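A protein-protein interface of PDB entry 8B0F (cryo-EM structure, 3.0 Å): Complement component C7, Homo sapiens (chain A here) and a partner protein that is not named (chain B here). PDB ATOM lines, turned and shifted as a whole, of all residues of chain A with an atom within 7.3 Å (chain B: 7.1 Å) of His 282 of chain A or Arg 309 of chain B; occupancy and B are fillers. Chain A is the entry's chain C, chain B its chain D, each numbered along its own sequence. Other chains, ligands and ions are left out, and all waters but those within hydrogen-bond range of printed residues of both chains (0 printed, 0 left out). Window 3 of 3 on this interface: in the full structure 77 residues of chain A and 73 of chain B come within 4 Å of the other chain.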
ATOM      1  N   ASN A  40     -17.829  17.572  -3.573  1.00  0.00           N
ATOM      2  CA  ASN A  40     -17.459  18.954  -3.861  1.00  0.00           C
ATOM      3  C   ASN A  40     -18.239  19.923  -2.977  1.00  0.00           C
ATOM      4  O   ASN A  40     -19.472  19.960  -3.014  1.00  0.00           O
ATOM      5  CB  ASN A  40     -17.711  19.248  -5.338  1.00  0.00           C
ATOM      6  CG  ASN A  40     -17.198  20.603  -5.761  1.00  0.00           C
ATOM      7  OD1 ASN A  40     -16.755  21.398  -4.938  1.00  0.00           O
ATOM      8  ND2 ASN A  40     -17.261  20.876  -7.057  1.00  0.00           N
ATOM      9  N   CYS A  42     -18.258  23.142  -3.480  1.00  0.00           N
ATOM     10  CA  CYS A  42     -18.856  24.150  -4.357  1.00  0.00           C
ATOM     11  C   CYS A  42     -20.150  23.692  -5.011  1.00  0.00           C
ATOM     12  O   CYS A  42     -21.003  24.531  -5.323  1.00  0.00           O
ATOM     13  CB  CYS A  42     -17.854  24.588  -5.421  1.00  0.00           C
ATOM     14  SG  CYS A  42     -16.291  25.168  -4.747  1.00  0.00           S
ATOM     15  N   THR A  43     -20.330  22.393  -5.234  1.00  0.00           N
ATOM     16  CA  THR A  43     -21.454  21.922  -6.029  1.00  0.00           C
ATOM     17  C   THR A  43     -22.232  20.796  -5.373  1.00  0.00           C
ATOM     18  O   THR A  43     -23.242  20.365  -5.935  1.00  0.00           O
ATOM     19  CB  THR A  43     -20.979  21.456  -7.414  1.00  0.00           C
ATOM     20  OG1 THR A  43     -20.303  20.200  -7.295  1.00  0.00           O
ATOM     21  CG2 THR A  43     -20.048  22.481  -8.038  1.00  0.00           C
ATOM     22  N   PRO A 275     -11.355  33.035 -20.619  1.00  0.00           N
ATOM     23  CA  PRO A 275     -12.148  31.801 -20.467  1.00  0.00           C
ATOM     24  C   PRO A 275     -11.381  30.621 -19.895  1.00  0.00           C
ATOM     25  O   PRO A 275     -11.948  29.844 -19.118  1.00  0.00           O
ATOM     26  CB  PRO A 275     -12.638  31.528 -21.897  1.00  0.00           C
ATOM     27  CG  PRO A 275     -11.706  32.262 -22.780  1.00  0.00           C
ATOM     28  CD  PRO A 275     -11.305  33.481 -22.018  1.00  0.00           C
ATOM     29  N   PHE A 276     -10.104  30.462 -20.235  1.00  0.00           N
ATOM     30  CA  PHE A 276      -9.314  29.391 -19.633  1.00  0.00           C
ATOM     31  C   PHE A 276      -9.170  29.595 -18.132  1.00  0.00           C
ATOM     32  O   PHE A 276      -9.321  28.655 -17.346  1.00  0.00           O
ATOM     33  CB  PHE A 276      -7.942  29.306 -20.296  1.00  0.00           C
ATOM     34  CG  PHE A 276      -7.071  28.224 -19.732  1.00  0.00           C
ATOM     35  CD1 PHE A 276      -7.516  26.920 -19.684  1.00  0.00           C
ATOM     36  CD2 PHE A 276      -5.803  28.508 -19.267  1.00  0.00           C
ATOM     37  CE1 PHE A 276      -6.719  25.925 -19.174  1.00  0.00           C
ATOM     38  CE2 PHE A 276      -5.003  27.512 -18.759  1.00  0.00           C
ATOM     39  CZ  PHE A 276      -5.462  26.220 -18.715  1.00  0.00           C
ATOM     40  N   TRP A 277      -8.837  30.815 -17.721  1.00  0.00           N
ATOM     41  CA  TRP A 277      -8.754  31.124 -16.300  1.00  0.00           C
ATOM     42  C   TRP A 277     -10.094  30.919 -15.601  1.00  0.00           C
ATOM     43  O   TRP A 277     -10.137  30.457 -14.457  1.00  0.00           O
ATOM     44  CB  TRP A 277      -8.273  32.561 -16.116  1.00  0.00           C
ATOM     45  CG  TRP A 277      -8.326  33.018 -14.706  1.00  0.00           C
ATOM     46  CD1 TRP A 277      -7.367  32.853 -13.755  1.00  0.00           C
ATOM     47  CD2 TRP A 277      -9.399  33.721 -14.079  1.00  0.00           C
ATOM     48  NE1 TRP A 277      -7.769  33.425 -12.576  1.00  0.00           N
ATOM     49  CE2 TRP A 277      -9.027  33.943 -12.742  1.00  0.00           C
ATOM     50  CE3 TRP A 277     -10.659  34.146 -14.506  1.00  0.00           C
ATOM     51  CZ2 TRP A 277      -9.851  34.598 -11.840  1.00  0.00           C
ATOM     52  CZ3 TRP A 277     -11.463  34.817 -13.618  1.00  0.00           C
ATOM     53  CH2 TRP A 277     -11.072  35.010 -12.291  1.00  0.00           C
ATOM     54  N   LYS A 278     -11.194  31.269 -16.264  1.00  0.00           N
ATOM     55  CA  LYS A 278     -12.523  30.975 -15.733  1.00  0.00           C
ATOM     56  C   LYS A 278     -12.757  29.482 -15.539  1.00  0.00           C
ATOM     57  O   LYS A 278     -13.353  29.070 -14.538  1.00  0.00           O
ATOM     58  CB  LYS A 278     -13.587  31.544 -16.668  1.00  0.00           C
ATOM     59  CG  LYS A 278     -13.717  33.051 -16.631  1.00  0.00           C
ATOM     60  CD  LYS A 278     -14.652  33.501 -15.523  1.00  0.00           C
ATOM     61  CE  LYS A 278     -16.107  33.233 -15.880  1.00  0.00           C
ATOM     62  NZ  LYS A 278     -17.047  33.816 -14.884  1.00  0.00           N
ATOM     63  N   GLU A 279     -12.312  28.655 -16.482  1.00  0.00           N
ATOM     64  CA  GLU A 279     -12.479  27.214 -16.311  1.00  0.00           C
ATOM     65  C   GLU A 279     -11.596  26.668 -15.194  1.00  0.00           C
ATOM     66  O   GLU A 279     -12.020  25.787 -14.440  1.00  0.00           O
ATOM     67  CB  GLU A 279     -12.175  26.499 -17.625  1.00  0.00           C
ATOM     68  CG  GLU A 279     -13.186  26.766 -18.732  1.00  0.00           C
ATOM     69  CD  GLU A 279     -14.621  26.561 -18.290  1.00  0.00           C
ATOM     70  OE1 GLU A 279     -15.005  25.403 -18.026  1.00  0.00           O
ATOM     71  OE2 GLU A 279     -15.365  27.559 -18.202  1.00  0.00           O
ATOM     72  N   LEU A 280     -10.369  27.171 -15.075  1.00  0.00           N
ATOM     73  CA  LEU A 280      -9.534  26.839 -13.922  1.00  0.00           C
ATOM     74  C   LEU A 280     -10.203  27.224 -12.609  1.00  0.00           C
ATOM     75  O   LEU A 280     -10.185  26.456 -11.642  1.00  0.00           O
ATOM     76  CB  LEU A 280      -8.174  27.524 -14.038  1.00  0.00           C
ATOM     77  CG  LEU A 280      -7.310  27.151 -15.238  1.00  0.00           C
ATOM     78  CD1 LEU A 280      -6.016  27.933 -15.193  1.00  0.00           C
ATOM     79  CD2 LEU A 280      -7.035  25.662 -15.267  1.00  0.00           C
ATOM     80  N   SER A 281     -10.795  28.415 -12.560  1.00  0.00           N
ATOM     81  CA  SER A 281     -11.521  28.862 -11.377  1.00  0.00           C
ATOM     82  C   SER A 281     -12.627  27.892 -10.981  1.00  0.00           C
ATOM     83  O   SER A 281     -12.860  27.668  -9.788  1.00  0.00           O
ATOM     84  CB  SER A 281     -12.102  30.252 -11.627  1.00  0.00           C
ATOM     85  OG  SER A 281     -12.661  30.786 -10.444  1.00  0.00           O
ATOM     86  N   HIS A 282     -13.320  27.314 -11.951  1.00  0.00           N
ATOM     87  CA  HIS A 282     -14.420  26.403 -11.667  1.00  0.00           C
ATOM     88  C   HIS A 282     -13.987  24.954 -11.481  1.00  0.00           C
ATOM     89  O   HIS A 282     -14.839  24.109 -11.193  1.00  0.00           O
ATOM     90  CB  HIS A 282     -15.463  26.488 -12.780  1.00  0.00           C
ATOM     91  CG  HIS A 282     -16.264  27.752 -12.749  1.00  0.00           C
ATOM     92  ND1 HIS A 282     -15.834  28.919 -13.339  1.00  0.00           N
ATOM     93  CD2 HIS A 282     -17.475  28.025 -12.210  1.00  0.00           C
ATOM     94  CE1 HIS A 282     -16.738  29.864 -13.150  1.00  0.00           C
ATOM     95  NE2 HIS A 282     -17.740  29.349 -12.463  1.00  0.00           N
ATOM     96  N   LEU A 283     -12.710  24.637 -11.647  1.00  0.00           N
ATOM     97  CA  LEU A 283     -12.244  23.309 -11.286  1.00  0.00           C
ATOM     98  C   LEU A 283     -12.528  23.052  -9.807  1.00  0.00           C
ATOM     99  O   LEU A 283     -12.386  23.960  -8.981  1.00  0.00           O
ATOM    100  CB  LEU A 283     -10.753  23.143 -11.574  1.00  0.00           C
ATOM    101  CG  LEU A 283     -10.348  23.177 -13.046  1.00  0.00           C
ATOM    102  CD1 LEU A 283      -8.844  23.316 -13.173  1.00  0.00           C
ATOM    103  CD2 LEU A 283     -10.828  21.932 -13.761  1.00  0.00           C
ATOM    104  N   PRO A 284     -12.933  21.834  -9.440  1.00  0.00           N
ATOM    105  CA  PRO A 284     -13.558  21.608  -8.128  1.00  0.00           C
ATOM    106  C   PRO A 284     -12.608  21.626  -6.937  1.00  0.00           C
ATOM    107  O   PRO A 284     -13.085  21.507  -5.804  1.00  0.00           O
ATOM    108  CB  PRO A 284     -14.200  20.228  -8.294  1.00  0.00           C
ATOM    109  CG  PRO A 284     -13.371  19.557  -9.303  1.00  0.00           C
ATOM    110  CD  PRO A 284     -12.938  20.614 -10.261  1.00  0.00           C
ATOM    111  N   SER A 285     -11.297  21.763  -7.125  1.00  0.00           N
ATOM    112  CA  SER A 285     -10.328  21.707  -6.033  1.00  0.00           C
ATOM    113  C   SER A 285     -10.233  20.324  -5.401  1.00  0.00           C
ATOM    114  O   SER A 285      -9.823  20.193  -4.246  1.00  0.00           O
ATOM    115  CB  SER A 285     -10.652  22.738  -4.945  1.00  0.00           C
ATOM    116  OG  SER A 285     -10.934  24.003  -5.509  1.00  0.00           O
ATOM    117  N   ALA A 291     -14.234  16.818 -14.378  1.00  0.00           N
ATOM    118  CA  ALA A 291     -13.976  18.231 -14.649  1.00  0.00           C
ATOM    119  C   ALA A 291     -12.635  18.450 -15.337  1.00  0.00           C
ATOM    120  O   ALA A 291     -12.544  19.165 -16.344  1.00  0.00           O
ATOM    121  CB  ALA A 291     -14.039  19.026 -13.347  1.00  0.00           C
ATOM    122  N   ARG A 294     -12.845  17.307 -18.862  1.00  0.00           N
ATOM    123  CA  ARG A 294     -13.489  18.322 -19.696  1.00  0.00           C
ATOM    124  C   ARG A 294     -12.555  19.490 -19.998  1.00  0.00           C
ATOM    125  O   ARG A 294     -12.571  20.041 -21.109  1.00  0.00           O
ATOM    126  CB  ARG A 294     -14.742  18.835 -18.992  1.00  0.00           C
ATOM    127  CG  ARG A 294     -15.678  19.641 -19.864  1.00  0.00           C
ATOM    128  CD  ARG A 294     -16.901  20.081 -19.074  1.00  0.00           C
ATOM    129  NE  ARG A 294     -17.604  18.955 -18.472  1.00  0.00           N
ATOM    130  CZ  ARG A 294     -18.318  18.065 -19.149  1.00  0.00           C
ATOM    131  NH1 ARG A 294     -18.554  18.207 -20.444  1.00  0.00           N
ATOM    132  NH2 ARG A 294     -18.837  17.025 -18.503  1.00  0.00           N
ATOM    133  N   GLN A 298     -11.236  20.480 -23.789  1.00  0.00           N
ATOM    134  CA  GLN A 298     -11.334  21.779 -24.454  1.00  0.00           C
ATOM    135  C   GLN A 298      -9.974  22.393 -24.773  1.00  0.00           C
ATOM    136  O   GLN A 298      -9.805  22.992 -25.839  1.00  0.00           O
ATOM    137  CB  GLN A 298     -12.138  22.745 -23.589  1.00  0.00           C
ATOM    138  CG  GLN A 298     -13.590  22.368 -23.423  1.00  0.00           C
ATOM    139  CD  GLN A 298     -14.345  23.367 -22.577  1.00  0.00           C
ATOM    140  OE1 GLN A 298     -14.922  24.323 -23.092  1.00  0.00           O
ATOM    141  NE2 GLN A 298     -14.339  23.156 -21.267  1.00  0.00           N
ATOM    142  N   VAL A 431      -5.600  31.341  -9.305  1.00  0.00           N
ATOM    143  CA  VAL A 431      -6.915  30.813  -8.936  1.00  0.00           C
ATOM    144  C   VAL A 431      -6.874  30.311  -7.496  1.00  0.00           C
ATOM    145  O   VAL A 431      -5.805  29.925  -7.003  1.00  0.00           O
ATOM    146  CB  VAL A 431      -7.381  29.701  -9.890  1.00  0.00           C
ATOM    147  CG1 VAL A 431      -7.531  30.232 -11.299  1.00  0.00           C
ATOM    148  CG2 VAL A 431      -6.414  28.530  -9.867  1.00  0.00           C
ATOM    149  N   PRO A 432      -7.999  30.314  -6.787  1.00  0.00           N
ATOM    150  CA  PRO A 432      -8.071  29.606  -5.506  1.00  0.00           C
ATOM    151  C   PRO A 432      -7.593  28.166  -5.626  1.00  0.00           C
ATOM    152  O   PRO A 432      -7.922  27.460  -6.579  1.00  0.00           O
ATOM    153  CB  PRO A 432      -9.557  29.679  -5.140  1.00  0.00           C
ATOM    154  CG  PRO A 432     -10.095  30.812  -5.928  1.00  0.00           C
ATOM    155  CD  PRO A 432      -9.312  30.840  -7.195  1.00  0.00           C
ATOM    156  N   LYS A 437      -4.961  22.361  -7.400  1.00  0.00           N
ATOM    157  CA  LYS A 437      -5.457  22.118  -8.750  1.00  0.00           C
ATOM    158  C   LYS A 437      -4.341  21.756  -9.719  1.00  0.00           C
ATOM    159  O   LYS A 437      -4.553  20.974 -10.643  1.00  0.00           O
ATOM    160  CB  LYS A 437      -6.233  23.330  -9.262  1.00  0.00           C
ATOM    161  CG  LYS A 437      -7.497  23.620  -8.482  1.00  0.00           C
ATOM    162  CD  LYS A 437      -8.138  24.919  -8.923  1.00  0.00           C
ATOM    163  CE  LYS A 437      -9.431  25.172  -8.175  1.00  0.00           C
ATOM    164  NZ  LYS A 437      -9.979  26.533  -8.415  1.00  0.00           N
ATOM    165  N   TYR B 214     -18.843  38.673 -27.707  1.00  0.00           N
ATOM    166  CA  TYR B 214     -18.604  38.194 -26.352  1.00  0.00           C
ATOM    167  C   TYR B 214     -18.851  36.699 -26.230  1.00  0.00           C
ATOM    168  O   TYR B 214     -18.161  36.016 -25.469  1.00  0.00           O
ATOM    169  CB  TYR B 214     -19.492  38.947 -25.366  1.00  0.00           C
ATOM    170  CG  TYR B 214     -19.669  38.229 -24.050  1.00  0.00           C
ATOM    171  CD1 TYR B 214     -18.755  38.386 -23.023  1.00  0.00           C
ATOM    172  CD2 TYR B 214     -20.749  37.385 -23.839  1.00  0.00           C
ATOM    173  CE1 TYR B 214     -18.924  37.747 -21.817  1.00  0.00           C
ATOM    174  CE2 TYR B 214     -20.918  36.730 -22.640  1.00  0.00           C
ATOM    175  CZ  TYR B 214     -20.005  36.916 -21.634  1.00  0.00           C
ATOM    176  OH  TYR B 214     -20.149  36.238 -20.448  1.00  0.00           O
ATOM    177  N   ASN B 215     -19.830  36.174 -26.966  1.00  0.00           N
ATOM    178  CA  ASN B 215     -20.154  34.754 -26.900  1.00  0.00           C
ATOM    179  C   ASN B 215     -19.043  33.864 -27.433  1.00  0.00           C
ATOM    180  O   ASN B 215     -19.050  32.664 -27.154  1.00  0.00           O
ATOM    181  CB  ASN B 215     -21.437  34.477 -27.679  1.00  0.00           C
ATOM    182  CG  ASN B 215     -22.674  34.708 -26.856  1.00  0.00           C
ATOM    183  OD1 ASN B 215     -22.858  34.092 -25.811  1.00  0.00           O
ATOM    184  ND2 ASN B 215     -23.547  35.581 -27.331  1.00  0.00           N
ATOM    185  N   LYS B 305     -14.830  28.450 -31.879  1.00  0.00           N
ATOM    186  CA  LYS B 305     -15.332  27.895 -30.630  1.00  0.00           C
ATOM    187  C   LYS B 305     -16.178  28.907 -29.876  1.00  0.00           C
ATOM    188  O   LYS B 305     -15.818  30.082 -29.770  1.00  0.00           O
ATOM    189  CB  LYS B 305     -14.220  27.419 -29.708  1.00  0.00           C
ATOM    190  CG  LYS B 305     -14.800  26.818 -28.442  1.00  0.00           C
ATOM    191  CD  LYS B 305     -13.851  25.917 -27.717  1.00  0.00           C
ATOM    192  CE  LYS B 305     -14.558  25.166 -26.614  1.00  0.00           C
ATOM    193  NZ  LYS B 305     -15.055  26.092 -25.566  1.00  0.00           N
ATOM    194  N   LEU B 306     -17.302  28.430 -29.355  1.00  0.00           N
ATOM    195  CA  LEU B 306     -18.127  29.201 -28.441  1.00  0.00           C
ATOM    196  C   LEU B 306     -17.581  29.089 -27.023  1.00  0.00           C
ATOM    197  O   LEU B 306     -17.018  28.065 -26.634  1.00  0.00           O
ATOM    198  CB  LEU B 306     -19.567  28.694 -28.489  1.00  0.00           C
ATOM    199  CG  LEU B 306     -20.637  29.533 -27.807  1.00  0.00           C
ATOM    200  CD1 LEU B 306     -21.061  30.674 -28.705  1.00  0.00           C
ATOM    201  CD2 LEU B 306     -21.818  28.656 -27.450  1.00  0.00           C
ATOM    202  N   LYS B 307     -17.755  30.154 -26.247  1.00  0.00           N
ATOM    203  CA  LYS B 307     -17.321  30.119 -24.860  1.00  0.00           C
ATOM    204  C   LYS B 307     -18.073  29.038 -24.087  1.00  0.00           C
ATOM    205  O   LYS B 307     -19.240  28.755 -24.366  1.00  0.00           O
ATOM    206  CB  LYS B 307     -17.526  31.477 -24.197  1.00  0.00           C
ATOM    207  CG  LYS B 307     -16.631  32.560 -24.751  1.00  0.00           C
ATOM    208  CD  LYS B 307     -16.862  33.886 -24.058  1.00  0.00           C
ATOM    209  CE  LYS B 307     -16.206  33.931 -22.699  1.00  0.00           C
ATOM    210  NZ  LYS B 307     -16.140  35.319 -22.171  1.00  0.00           N
ATOM    211  N   PRO B 308     -17.422  28.418 -23.100  1.00  0.00           N
ATOM    212  CA  PRO B 308     -18.077  27.344 -22.343  1.00  0.00           C
ATOM    213  C   PRO B 308     -19.178  27.813 -21.412  1.00  0.00           C
ATOM    214  O   PRO B 308     -19.975  26.978 -20.969  1.00  0.00           O
ATOM    215  CB  PRO B 308     -16.922  26.716 -21.553  1.00  0.00           C
ATOM    216  CG  PRO B 308     -15.919  27.795 -21.433  1.00  0.00           C
ATOM    217  CD  PRO B 308     -16.020  28.598 -22.691  1.00  0.00           C
ATOM    218  N   ARG B 309     -19.258  29.102 -21.092  1.00  0.00           N
ATOM    219  CA  ARG B 309     -19.964  29.523 -19.891  1.00  0.00           C
ATOM    220  C   ARG B 309     -20.521  30.927 -20.060  1.00  0.00           C
ATOM    221  O   ARG B 309     -19.972  31.751 -20.795  1.00  0.00           O
ATOM    222  CB  ARG B 309     -19.029  29.477 -18.680  1.00  0.00           C
ATOM    223  CG  ARG B 309     -19.732  29.411 -17.344  1.00  0.00           C
ATOM    224  CD  ARG B 309     -18.730  29.258 -16.215  1.00  0.00           C
ATOM    225  NE  ARG B 309     -17.963  28.024 -16.325  1.00  0.00           N
ATOM    226  CZ  ARG B 309     -18.372  26.842 -15.886  1.00  0.00           C
ATOM    227  NH1 ARG B 309     -19.509  26.703 -15.225  1.00  0.00           N
ATOM    228  NH2 ARG B 309     -17.613  25.772 -16.103  1.00  0.00           N
ATOM    229  N   SER B 310     -21.621  31.186 -19.352  1.00  0.00           N
ATOM    230  CA  SER B 310     -22.187  32.527 -19.207  1.00  0.00           C
ATOM    231  C   SER B 310     -22.479  33.169 -20.562  1.00  0.00           C
ATOM    232  O   SER B 310     -22.085  34.301 -20.842  1.00  0.00           O
ATOM    233  CB  SER B 310     -21.257  33.412 -18.377  1.00  0.00           C
ATOM    234  OG  SER B 310     -21.941  34.550 -17.884  1.00  0.00           O
ATOM    235  N   LEU B 311     -23.182  32.425 -21.409  1.00  0.00           N
ATOM    236  CA  LEU B 311     -23.511  32.879 -22.750  1.00  0.00           C
ATOM    237  C   LEU B 311     -24.644  33.897 -22.698  1.00  0.00           C
ATOM    238  O   LEU B 311     -25.504  33.852 -21.817  1.00  0.00           O
ATOM    239  CB  LEU B 311     -23.913  31.695 -23.625  1.00  0.00           C
ATOM    240  CG  LEU B 311     -22.816  30.664 -23.875  1.00  0.00           C
ATOM    241  CD1 LEU B 311     -23.406  29.421 -24.499  1.00  0.00           C
ATOM    242  CD2 LEU B 311     -21.727  31.240 -24.753  1.00  0.00           C
ATOM    243  N   MET B 312     -24.644  34.823 -23.657  1.00  0.00           N
ATOM    244  CA  MET B 312     -25.742  35.769 -23.829  1.00  0.00           C
ATOM    245  C   MET B 312     -26.693  35.221 -24.886  1.00  0.00           C
ATOM    246  O   MET B 312     -26.332  35.107 -26.059  1.00  0.00           O
ATOM    247  CB  MET B 312     -25.220  37.148 -24.223  1.00  0.00           C
ATOM    248  CG  MET B 312     -26.306  38.206 -24.351  1.00  0.00           C
ATOM    249  SD  MET B 312     -27.190  38.506 -22.809  1.00  0.00           S
ATOM    250  CE  MET B 312     -25.969  39.426 -21.885  1.00  0.00           C
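Of the 20 printed residues of chain A, 3 touch a printed residue of chain B.
Printed residues of chain A that touch a printed residue of chain B: Glu 279, His 282 and Gln 298.
Hydrophobic or aromatic side chains of chain A that line the printed part of chain B: His 282.
Along chain A the printed residues that touch a printed residue of chain B span positions 279 to 298.
Hydrophobic or aromatic side chains of chain B within 4 Å of the printed part of chain A: Pro 308.
Among the printed residues, Asp or Glu carboxylates within 4 Å of a Lys or Arg side-chain nitrogen of the other chain: Glu 279 of chain A with Arg 309 of chain B (3.2 Å).
The side-chain carboxylate of Glu 279 of chain A lies within salt-bridge range of the guanidinium group of Arg 309 of chain B, at 3.2 Å.
The side-chain amide oxygen of Gln 298 of chain A sits at hydrogen-bond distance from the side-chain amino group of Lys 305 of chain B.
His 282 of chain A touches just one residue of chain B: Arg 309 (3.7 Å).
Arg 309 of chain B touches two residues of chain A.
Printed residues of chain A within 4 Å of Pro 308 of chain B: Glu 279 and Gln 298.
Of the printed residues of chain B, Glu 279 of chain A touches Pro 308 (3.3 Å) and Arg 309 (3.2 Å).
Arg 294 of chain A touches none of the printed residues of chain B.
O of Lys 278 of chain A lies within hydrogen-bond range of ND1 of His 282 of chain A, 2.8 Å away.
Pro 308 of chain B touches Glu 279 of chain A (CG to OE2, 3.3 Å).
His 282 of chain A touches Arg 309 of chain B (CE1 to CD, 3.7 Å).
Pro 308 of chain B touches Gln 298 of chain A.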
